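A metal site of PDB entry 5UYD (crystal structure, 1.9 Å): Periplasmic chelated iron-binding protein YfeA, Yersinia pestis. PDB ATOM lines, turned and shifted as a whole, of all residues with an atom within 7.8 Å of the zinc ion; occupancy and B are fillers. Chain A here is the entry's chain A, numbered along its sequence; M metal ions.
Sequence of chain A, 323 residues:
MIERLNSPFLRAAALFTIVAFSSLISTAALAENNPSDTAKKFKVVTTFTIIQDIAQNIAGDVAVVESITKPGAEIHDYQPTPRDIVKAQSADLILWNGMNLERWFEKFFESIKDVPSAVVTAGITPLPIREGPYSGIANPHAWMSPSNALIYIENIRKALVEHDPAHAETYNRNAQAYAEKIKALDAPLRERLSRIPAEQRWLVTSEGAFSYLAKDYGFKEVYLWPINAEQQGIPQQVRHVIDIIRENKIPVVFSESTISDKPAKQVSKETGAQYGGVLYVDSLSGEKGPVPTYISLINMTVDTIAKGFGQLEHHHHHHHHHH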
ATOM      1  N   GLU A  74     -15.152  -6.136  30.332  1.00  0.00           N
ATOM      2  CA  GLU A  74     -15.687  -7.015  29.299  1.00  0.00           C
ATOM      3  C   GLU A  74     -15.179  -6.547  27.936  1.00  0.00           C
ATOM      4  O   GLU A  74     -15.330  -5.377  27.569  1.00  0.00           O
ATOM      5  CB  GLU A  74     -17.212  -6.983  29.369  1.00  0.00           C
ATOM      6  CG  GLU A  74     -17.904  -8.158  28.729  1.00  0.00           C
ATOM      7  CD  GLU A  74     -17.702  -8.165  27.237  1.00  0.00           C
ATOM      8  OE1 GLU A  74     -18.133  -7.204  26.562  1.00  0.00           O
ATOM      9  OE2 GLU A  74     -17.070  -9.123  26.749  1.00  0.00           O
ATOM     10  N   ILE A  75     -14.543  -7.452  27.184  1.00  0.00           N
ATOM     11  CA  ILE A  75     -13.778  -7.042  25.995  1.00  0.00           C
ATOM     12  C   ILE A  75     -14.532  -7.155  24.662  1.00  0.00           C
ATOM     13  O   ILE A  75     -14.128  -6.505  23.686  1.00  0.00           O
ATOM     14  CB  ILE A  75     -12.456  -7.831  25.891  1.00  0.00           C
ATOM     15  CG1 ILE A  75     -12.739  -9.303  25.583  1.00  0.00           C
ATOM     16  CG2 ILE A  75     -11.674  -7.700  27.174  1.00  0.00           C
ATOM     17  CD1 ILE A  75     -11.461 -10.156  25.396  1.00  0.00           C
ATOM     18  N   HIS A  76     -15.568  -7.998  24.574  1.00  0.00           N
ATOM     19  CA  HIS A  76     -16.248  -8.201  23.293  1.00  0.00           C
ATOM     20  C   HIS A  76     -16.976  -6.947  22.841  1.00  0.00           C
ATOM     21  O   HIS A  76     -16.852  -6.509  21.692  1.00  0.00           O
ATOM     22  CB  HIS A  76     -17.233  -9.358  23.396  1.00  0.00           C
ATOM     23  CG  HIS A  76     -16.594 -10.694  23.656  1.00  0.00           C
ATOM     24  ND1 HIS A  76     -16.466 -11.648  22.680  1.00  0.00           N
ATOM     25  CD2 HIS A  76     -16.079 -11.232  24.789  1.00  0.00           C
ATOM     26  CE1 HIS A  76     -15.891 -12.732  23.192  1.00  0.00           C
ATOM     27  NE2 HIS A  76     -15.656 -12.502  24.473  1.00  0.00           N
ATOM     28  N   LEU A 101     -13.435 -11.073  17.846  1.00  0.00           N
ATOM     29  CA  LEU A 101     -13.422 -10.812  19.287  1.00  0.00           C
ATOM     30  C   LEU A 101     -13.863  -9.377  19.552  1.00  0.00           C
ATOM     31  O   LEU A 101     -14.908  -9.143  20.176  1.00  0.00           O
ATOM     32  CB  LEU A 101     -12.025 -11.072  19.875  1.00  0.00           C
ATOM     33  CG  LEU A 101     -11.847 -10.734  21.356  1.00  0.00           C
ATOM     34  CD1 LEU A 101     -12.671 -11.670  22.288  1.00  0.00           C
ATOM     35  CD2 LEU A 101     -10.398 -10.764  21.737  1.00  0.00           C
ATOM     36  N   ASN A 139     -14.943 -18.761  16.681  1.00  0.00           N
ATOM     37  CA  ASN A 139     -14.815 -18.498  18.110  1.00  0.00           C
ATOM     38  C   ASN A 139     -13.503 -17.754  18.349  1.00  0.00           C
ATOM     39  O   ASN A 139     -12.439 -18.265  17.996  1.00  0.00           O
ATOM     40  CB  ASN A 139     -14.840 -19.835  18.865  1.00  0.00           C
ATOM     41  CG  ASN A 139     -14.903 -19.678  20.382  1.00  0.00           C
ATOM     42  OD1 ASN A 139     -14.255 -18.800  20.965  1.00  0.00           O
ATOM     43  ND2 ASN A 139     -15.674 -20.550  21.035  1.00  0.00           N
ATOM     44  N   PRO A 140     -13.531 -16.551  18.945  1.00  0.00           N
ATOM     45  CA  PRO A 140     -12.281 -15.786  19.083  1.00  0.00           C
ATOM     46  C   PRO A 140     -11.313 -16.323  20.143  1.00  0.00           C
ATOM     47  O   PRO A 140     -10.137 -15.895  20.139  1.00  0.00           O
ATOM     48  CB  PRO A 140     -12.777 -14.387  19.478  1.00  0.00           C
ATOM     49  CG  PRO A 140     -14.089 -14.645  20.208  1.00  0.00           C
ATOM     50  CD  PRO A 140     -14.707 -15.791  19.406  1.00  0.00           C
ATOM     51  N   HIS A 141     -11.741 -17.188  21.069  1.00  0.00           N
ATOM     52  CA  HIS A 141     -10.932 -17.434  22.270  1.00  0.00           C
ATOM     53  C   HIS A 141      -9.793 -18.417  22.018  1.00  0.00           C
ATOM     54  O   HIS A 141      -9.576 -19.331  22.828  1.00  0.00           O
ATOM     55  CB  HIS A 141     -11.820 -17.939  23.411  1.00  0.00           C
ATOM     56  CG  HIS A 141     -12.954 -17.017  23.753  1.00  0.00           C
ATOM     57  ND1 HIS A 141     -14.195 -17.115  23.158  1.00  0.00           N
ATOM     58  CD2 HIS A 141     -13.033 -15.980  24.624  1.00  0.00           C
ATOM     59  CE1 HIS A 141     -14.994 -16.185  23.661  1.00  0.00           C
ATOM     60  NE2 HIS A 141     -14.318 -15.484  24.552  1.00  0.00           N
ATOM     61  N   TRP A 143      -6.607 -18.270  22.316  1.00  0.00           N
ATOM     62  CA  TRP A 143      -5.461 -18.248  23.220  1.00  0.00           C
ATOM     63  C   TRP A 143      -5.591 -19.224  24.386  1.00  0.00           C
ATOM     64  O   TRP A 143      -4.606 -19.437  25.119  1.00  0.00           O
ATOM     65  CB  TRP A 143      -5.261 -16.823  23.783  1.00  0.00           C
ATOM     66  CG  TRP A 143      -6.436 -16.344  24.594  1.00  0.00           C
ATOM     67  CD1 TRP A 143      -6.664 -16.581  25.925  1.00  0.00           C
ATOM     68  CD2 TRP A 143      -7.551 -15.553  24.125  1.00  0.00           C
ATOM     69  NE1 TRP A 143      -7.850 -15.991  26.307  1.00  0.00           N
ATOM     70  CE2 TRP A 143      -8.418 -15.363  25.229  1.00  0.00           C
ATOM     71  CE3 TRP A 143      -7.903 -15.012  22.878  1.00  0.00           C
ATOM     72  CZ2 TRP A 143      -9.615 -14.632  25.128  1.00  0.00           C
ATOM     73  CZ3 TRP A 143      -9.092 -14.286  22.780  1.00  0.00           C
ATOM     74  CH2 TRP A 143      -9.932 -14.103  23.899  1.00  0.00           C
ATOM     75  N   GLU A 207     -19.989 -18.094  29.513  1.00  0.00           N
ATOM     76  CA  GLU A 207     -19.696 -17.925  28.094  1.00  0.00           C
ATOM     77  C   GLU A 207     -19.060 -19.208  27.567  1.00  0.00           C
ATOM     78  O   GLU A 207     -18.295 -19.872  28.272  1.00  0.00           O
ATOM     79  CB  GLU A 207     -18.754 -16.749  27.836  1.00  0.00           C
ATOM     80  CG  GLU A 207     -18.466 -16.519  26.327  1.00  0.00           C
ATOM     81  CD  GLU A 207     -17.502 -15.354  26.024  1.00  0.00           C
ATOM     82  OE1 GLU A 207     -16.591 -15.084  26.840  1.00  0.00           O
ATOM     83  OE2 GLU A 207     -17.655 -14.733  24.964  1.00  0.00           O
ATOM     84  N   GLY A 208     -19.392 -19.542  26.319  1.00  0.00           N
ATOM     85  CA  GLY A 208     -18.715 -20.650  25.626  1.00  0.00           C
ATOM     86  C   GLY A 208     -17.309 -20.278  25.194  1.00  0.00           C
ATOM     87  O   GLY A 208     -16.927 -20.449  24.017  1.00  0.00           O
ATOM     88  N   ALA A 209     -16.519 -19.785  26.138  1.00  0.00           N
ATOM     89  CA  ALA A 209     -15.192 -19.231  25.853  1.00  0.00           C
ATOM     90  C   ALA A 209     -14.092 -20.272  25.852  1.00  0.00           C
ATOM     91  O   ALA A 209     -12.945 -19.923  25.563  1.00  0.00           O
ATOM     92  CB  ALA A 209     -14.838 -18.147  26.881  1.00  0.00           C
ATOM     93  N   PHE A 210     -14.386 -21.529  26.166  1.00  0.00           N
ATOM     94  CA  PHE A 210     -13.325 -22.501  26.422  1.00  0.00           C
ATOM     95  C   PHE A 210     -13.217 -23.569  25.350  1.00  0.00           C
ATOM     96  O   PHE A 210     -12.566 -24.599  25.568  1.00  0.00           O
ATOM     97  CB  PHE A 210     -13.541 -23.116  27.809  1.00  0.00           C
ATOM     98  CG  PHE A 210     -13.516 -22.078  28.902  1.00  0.00           C
ATOM     99  CD1 PHE A 210     -12.304 -21.697  29.467  1.00  0.00           C
ATOM    100  CD2 PHE A 210     -14.668 -21.425  29.291  1.00  0.00           C
ATOM    101  CE1 PHE A 210     -12.256 -20.696  30.433  1.00  0.00           C
ATOM    102  CE2 PHE A 210     -14.624 -20.428  30.264  1.00  0.00           C
ATOM    103  CZ  PHE A 210     -13.414 -20.072  30.827  1.00  0.00           C
ATOM    104  N   TRP A 225     -24.242 -19.201  27.364  1.00  0.00           N
ATOM    105  CA  TRP A 225     -24.398 -18.430  26.119  1.00  0.00           C
ATOM    106  C   TRP A 225     -23.163 -18.633  25.254  1.00  0.00           C
ATOM    107  O   TRP A 225     -22.055 -18.760  25.784  1.00  0.00           O
ATOM    108  CB  TRP A 225     -24.627 -16.937  26.364  1.00  0.00           C
ATOM    109  CG  TRP A 225     -23.612 -16.234  27.224  1.00  0.00           C
ATOM    110  CD1 TRP A 225     -22.461 -15.598  26.822  1.00  0.00           C
ATOM    111  CD2 TRP A 225     -23.674 -16.070  28.651  1.00  0.00           C
ATOM    112  NE1 TRP A 225     -21.809 -15.063  27.912  1.00  0.00           N
ATOM    113  CE2 TRP A 225     -22.534 -15.335  29.048  1.00  0.00           C
ATOM    114  CE3 TRP A 225     -24.593 -16.471  29.641  1.00  0.00           C
ATOM    115  CZ2 TRP A 225     -22.277 -14.995  30.381  1.00  0.00           C
ATOM    116  CZ3 TRP A 225     -24.342 -16.129  30.958  1.00  0.00           C
ATOM    117  CH2 TRP A 225     -23.193 -15.404  31.315  1.00  0.00           C
ATOM    118  N   PRO A 226     -23.331 -18.692  23.931  1.00  0.00           N
ATOM    119  CA  PRO A 226     -22.194 -19.069  23.056  1.00  0.00           C
ATOM    120  C   PRO A 226     -21.084 -18.035  23.010  1.00  0.00           C
ATOM    121  O   PRO A 226     -19.907 -18.416  22.896  1.00  0.00           O
ATOM    122  CB  PRO A 226     -22.854 -19.253  21.679  1.00  0.00           C
ATOM    123  CG  PRO A 226     -24.214 -18.618  21.774  1.00  0.00           C
ATOM    124  CD  PRO A 226     -24.623 -18.704  23.215  1.00  0.00           C
ATOM    125  N   ILE A 227     -21.399 -16.749  23.086  1.00  0.00           N
ATOM    126  CA  ILE A 227     -20.380 -15.705  23.077  1.00  0.00           C
ATOM    127  C   ILE A 227     -20.998 -14.472  23.709  1.00  0.00           C
ATOM    128  O   ILE A 227     -22.197 -14.222  23.567  1.00  0.00           O
ATOM    129  CB  ILE A 227     -19.850 -15.450  21.644  1.00  0.00           C
ATOM    130  CG1 ILE A 227     -18.775 -14.359  21.621  1.00  0.00           C
ATOM    131  CG2 ILE A 227     -21.000 -15.105  20.709  1.00  0.00           C
ATOM    132  CD1 ILE A 227     -17.911 -14.347  20.349  1.00  0.00           C
ATOM    133  N   ASN A 228     -20.195 -13.723  24.460  1.00  0.00           N
ATOM    134  CA  ASN A 228     -20.708 -12.514  25.098  1.00  0.00           C
ATOM    135  C   ASN A 228     -21.378 -11.617  24.068  1.00  0.00           C
ATOM    136  O   ASN A 228     -20.829 -11.362  22.989  1.00  0.00           O
ATOM    137  CB  ASN A 228     -19.566 -11.757  25.795  1.00  0.00           C
ATOM    138  CG  ASN A 228     -19.019 -12.508  27.002  1.00  0.00           C
ATOM    139  OD1 ASN A 228     -19.540 -13.548  27.392  1.00  0.00           O
ATOM    140  ND2 ASN A 228     -17.976 -11.959  27.601  1.00  0.00           N
ATOM    141  N   GLU A 256     -16.926 -16.789  34.664  1.00  0.00           N
ATOM    142  CA  GLU A 256     -15.688 -16.190  34.193  1.00  0.00           C
ATOM    143  C   GLU A 256     -15.547 -14.772  34.737  1.00  0.00           C
ATOM    144  O   GLU A 256     -16.532 -14.133  35.113  1.00  0.00           O
ATOM    145  CB  GLU A 256     -15.602 -16.171  32.661  1.00  0.00           C
ATOM    146  CG  GLU A 256     -15.754 -17.568  32.013  1.00  0.00           C
ATOM    147  CD  GLU A 256     -17.215 -17.932  31.799  1.00  0.00           C
ATOM    148  OE1 GLU A 256     -17.928 -17.133  31.170  1.00  0.00           O
ATOM    149  OE2 GLU A 256     -17.636 -19.017  32.275  1.00  0.00           O
ATOM    150  N   THR A 258     -14.935 -11.695  33.711  1.00  0.00           N
ATOM    151  CA  THR A 258     -15.494 -10.441  33.229  1.00  0.00           C
ATOM    152  C   THR A 258     -17.014 -10.415  33.109  1.00  0.00           C
ATOM    153  O   THR A 258     -17.566  -9.411  32.673  1.00  0.00           O
ATOM    154  CB  THR A 258     -14.891 -10.041  31.865  1.00  0.00           C
ATOM    155  OG1 THR A 258     -15.429 -10.853  30.815  1.00  0.00           O
ATOM    156  CG2 THR A 258     -13.368 -10.105  31.884  1.00  0.00           C
ATOM    157  N   ILE A 259     -17.710 -11.488  33.492  1.00  0.00           N
ATOM    158  CA  ILE A 259     -19.158 -11.507  33.368  1.00  0.00           C
ATOM    159  C   ILE A 259     -19.775 -11.832  34.725  1.00  0.00           C
ATOM    160  O   ILE A 259     -19.051 -12.007  35.705  1.00  0.00           O
ATOM    161  CB  ILE A 259     -19.608 -12.489  32.266  1.00  0.00           C
ATOM    162  CG1 ILE A 259     -18.885 -13.841  32.399  1.00  0.00           C
ATOM    163  CG2 ILE A 259     -19.357 -11.880  30.873  1.00  0.00           C
ATOM    164  CD1 ILE A 259     -19.527 -14.796  33.434  1.00  0.00           C
ATOM    165  N   VAL A 281     -10.394 -16.018  31.359  1.00  0.00           N
ATOM    166  CA  VAL A 281     -10.269 -16.247  29.925  1.00  0.00           C
ATOM    167  C   VAL A 281     -10.150 -14.909  29.182  1.00  0.00           C
ATOM    168  O   VAL A 281      -9.213 -14.715  28.409  1.00  0.00           O
ATOM    169  CB  VAL A 281     -11.433 -17.092  29.378  1.00  0.00           C
ATOM    170  CG1 VAL A 281     -12.798 -16.587  29.883  1.00  0.00           C
ATOM    171  CG2 VAL A 281     -11.381 -17.136  27.839  1.00  0.00           C
ATOM    172  N   ASP A 282     -11.087 -13.979  29.424  1.00  0.00           N
ATOM    173  CA  ASP A 282     -11.113 -12.736  28.658  1.00  0.00           C
ATOM    174  C   ASP A 282     -10.259 -11.631  29.275  1.00  0.00           C
ATOM    175  O   ASP A 282     -10.030 -10.603  28.631  1.00  0.00           O
ATOM    176  CB  ASP A 282     -12.547 -12.205  28.517  1.00  0.00           C
ATOM    177  CG  ASP A 282     -13.357 -12.980  27.472  1.00  0.00           C
ATOM    178  OD1 ASP A 282     -12.788 -13.836  26.784  1.00  0.00           O
ATOM    179  OD2 ASP A 282     -14.574 -12.699  27.364  1.00  0.00           O
ATOM    180  N   SER A 283      -9.774 -11.814  30.502  1.00  0.00           N
ATOM    181  CA  SER A 283      -8.938 -10.776  31.095  1.00  0.00           C
ATOM    182  C   SER A 283      -8.009 -11.401  32.116  1.00  0.00           C
ATOM    183  O   SER A 283      -8.343 -12.406  32.754  1.00  0.00           O
ATOM    184  CB  SER A 283      -9.779  -9.662  31.744  1.00  0.00           C
ATOM    185  OG  SER A 283      -8.942  -8.693  32.391  1.00  0.00           O
HETATM  186 ZN    ZN M   1     -15.182 -14.008  25.794  1.00  0.00          ZN
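The side-chain amide nitrogen (ND2) of Asn 228 lies within hydrogen-bond range of the side-chain carboxylate (OE2) of Glu 74 (3.1 Å).
The backbone NH (N) of Glu 207 sits at hydrogen-bond distance from the side-chain carboxylate (OE1) of Glu 256 (2.8 Å).
OD1 of Asn 228 sits at hydrogen-bond distance from NE1 of Trp 225 (2.8 Å).
The side-chain carboxylate (OE2) of Glu 74 lies within hydrogen-bond range of the backbone NH (N) of His 76, 2.9 Å away.
N of Asn 228 is in hydrogen-bond range of OE2 of Glu 207, 2.8 Å away.
A ring nitrogen (ND1) of His 141 sits at hydrogen-bond distance from the side-chain amide oxygen of Asn 139, 2.8 Å away.
ND2 of Asn 228 lies close to OD2 of Asp 282, 3.5 Å away.
Merely in contact with the zinc ion: Asn 228 (3.9 Å).
Within 4 Å of the zinc ion: His 76, His 141, Glu 207, Asn 228 and Asp 282.
A ring nitrogen (NE2) of His 76 is bound to the zinc ion, 2.1 Å away.
The side-chain carboxylate (OE1) of Glu 207 binds the zinc ion (2.1 Å).
A ring nitrogen (NE2) of His 141 binds the zinc ion (2.1 Å).
OD2 of Asp 282 binds the zinc ion, at 2.1 Å.
OD1 of Asp 282 binds the zinc ion, 2.6 Å away.
Slightly farther from the zinc ion lies the side-chain carboxylate (OE2) of Glu 207 (2.7 Å).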
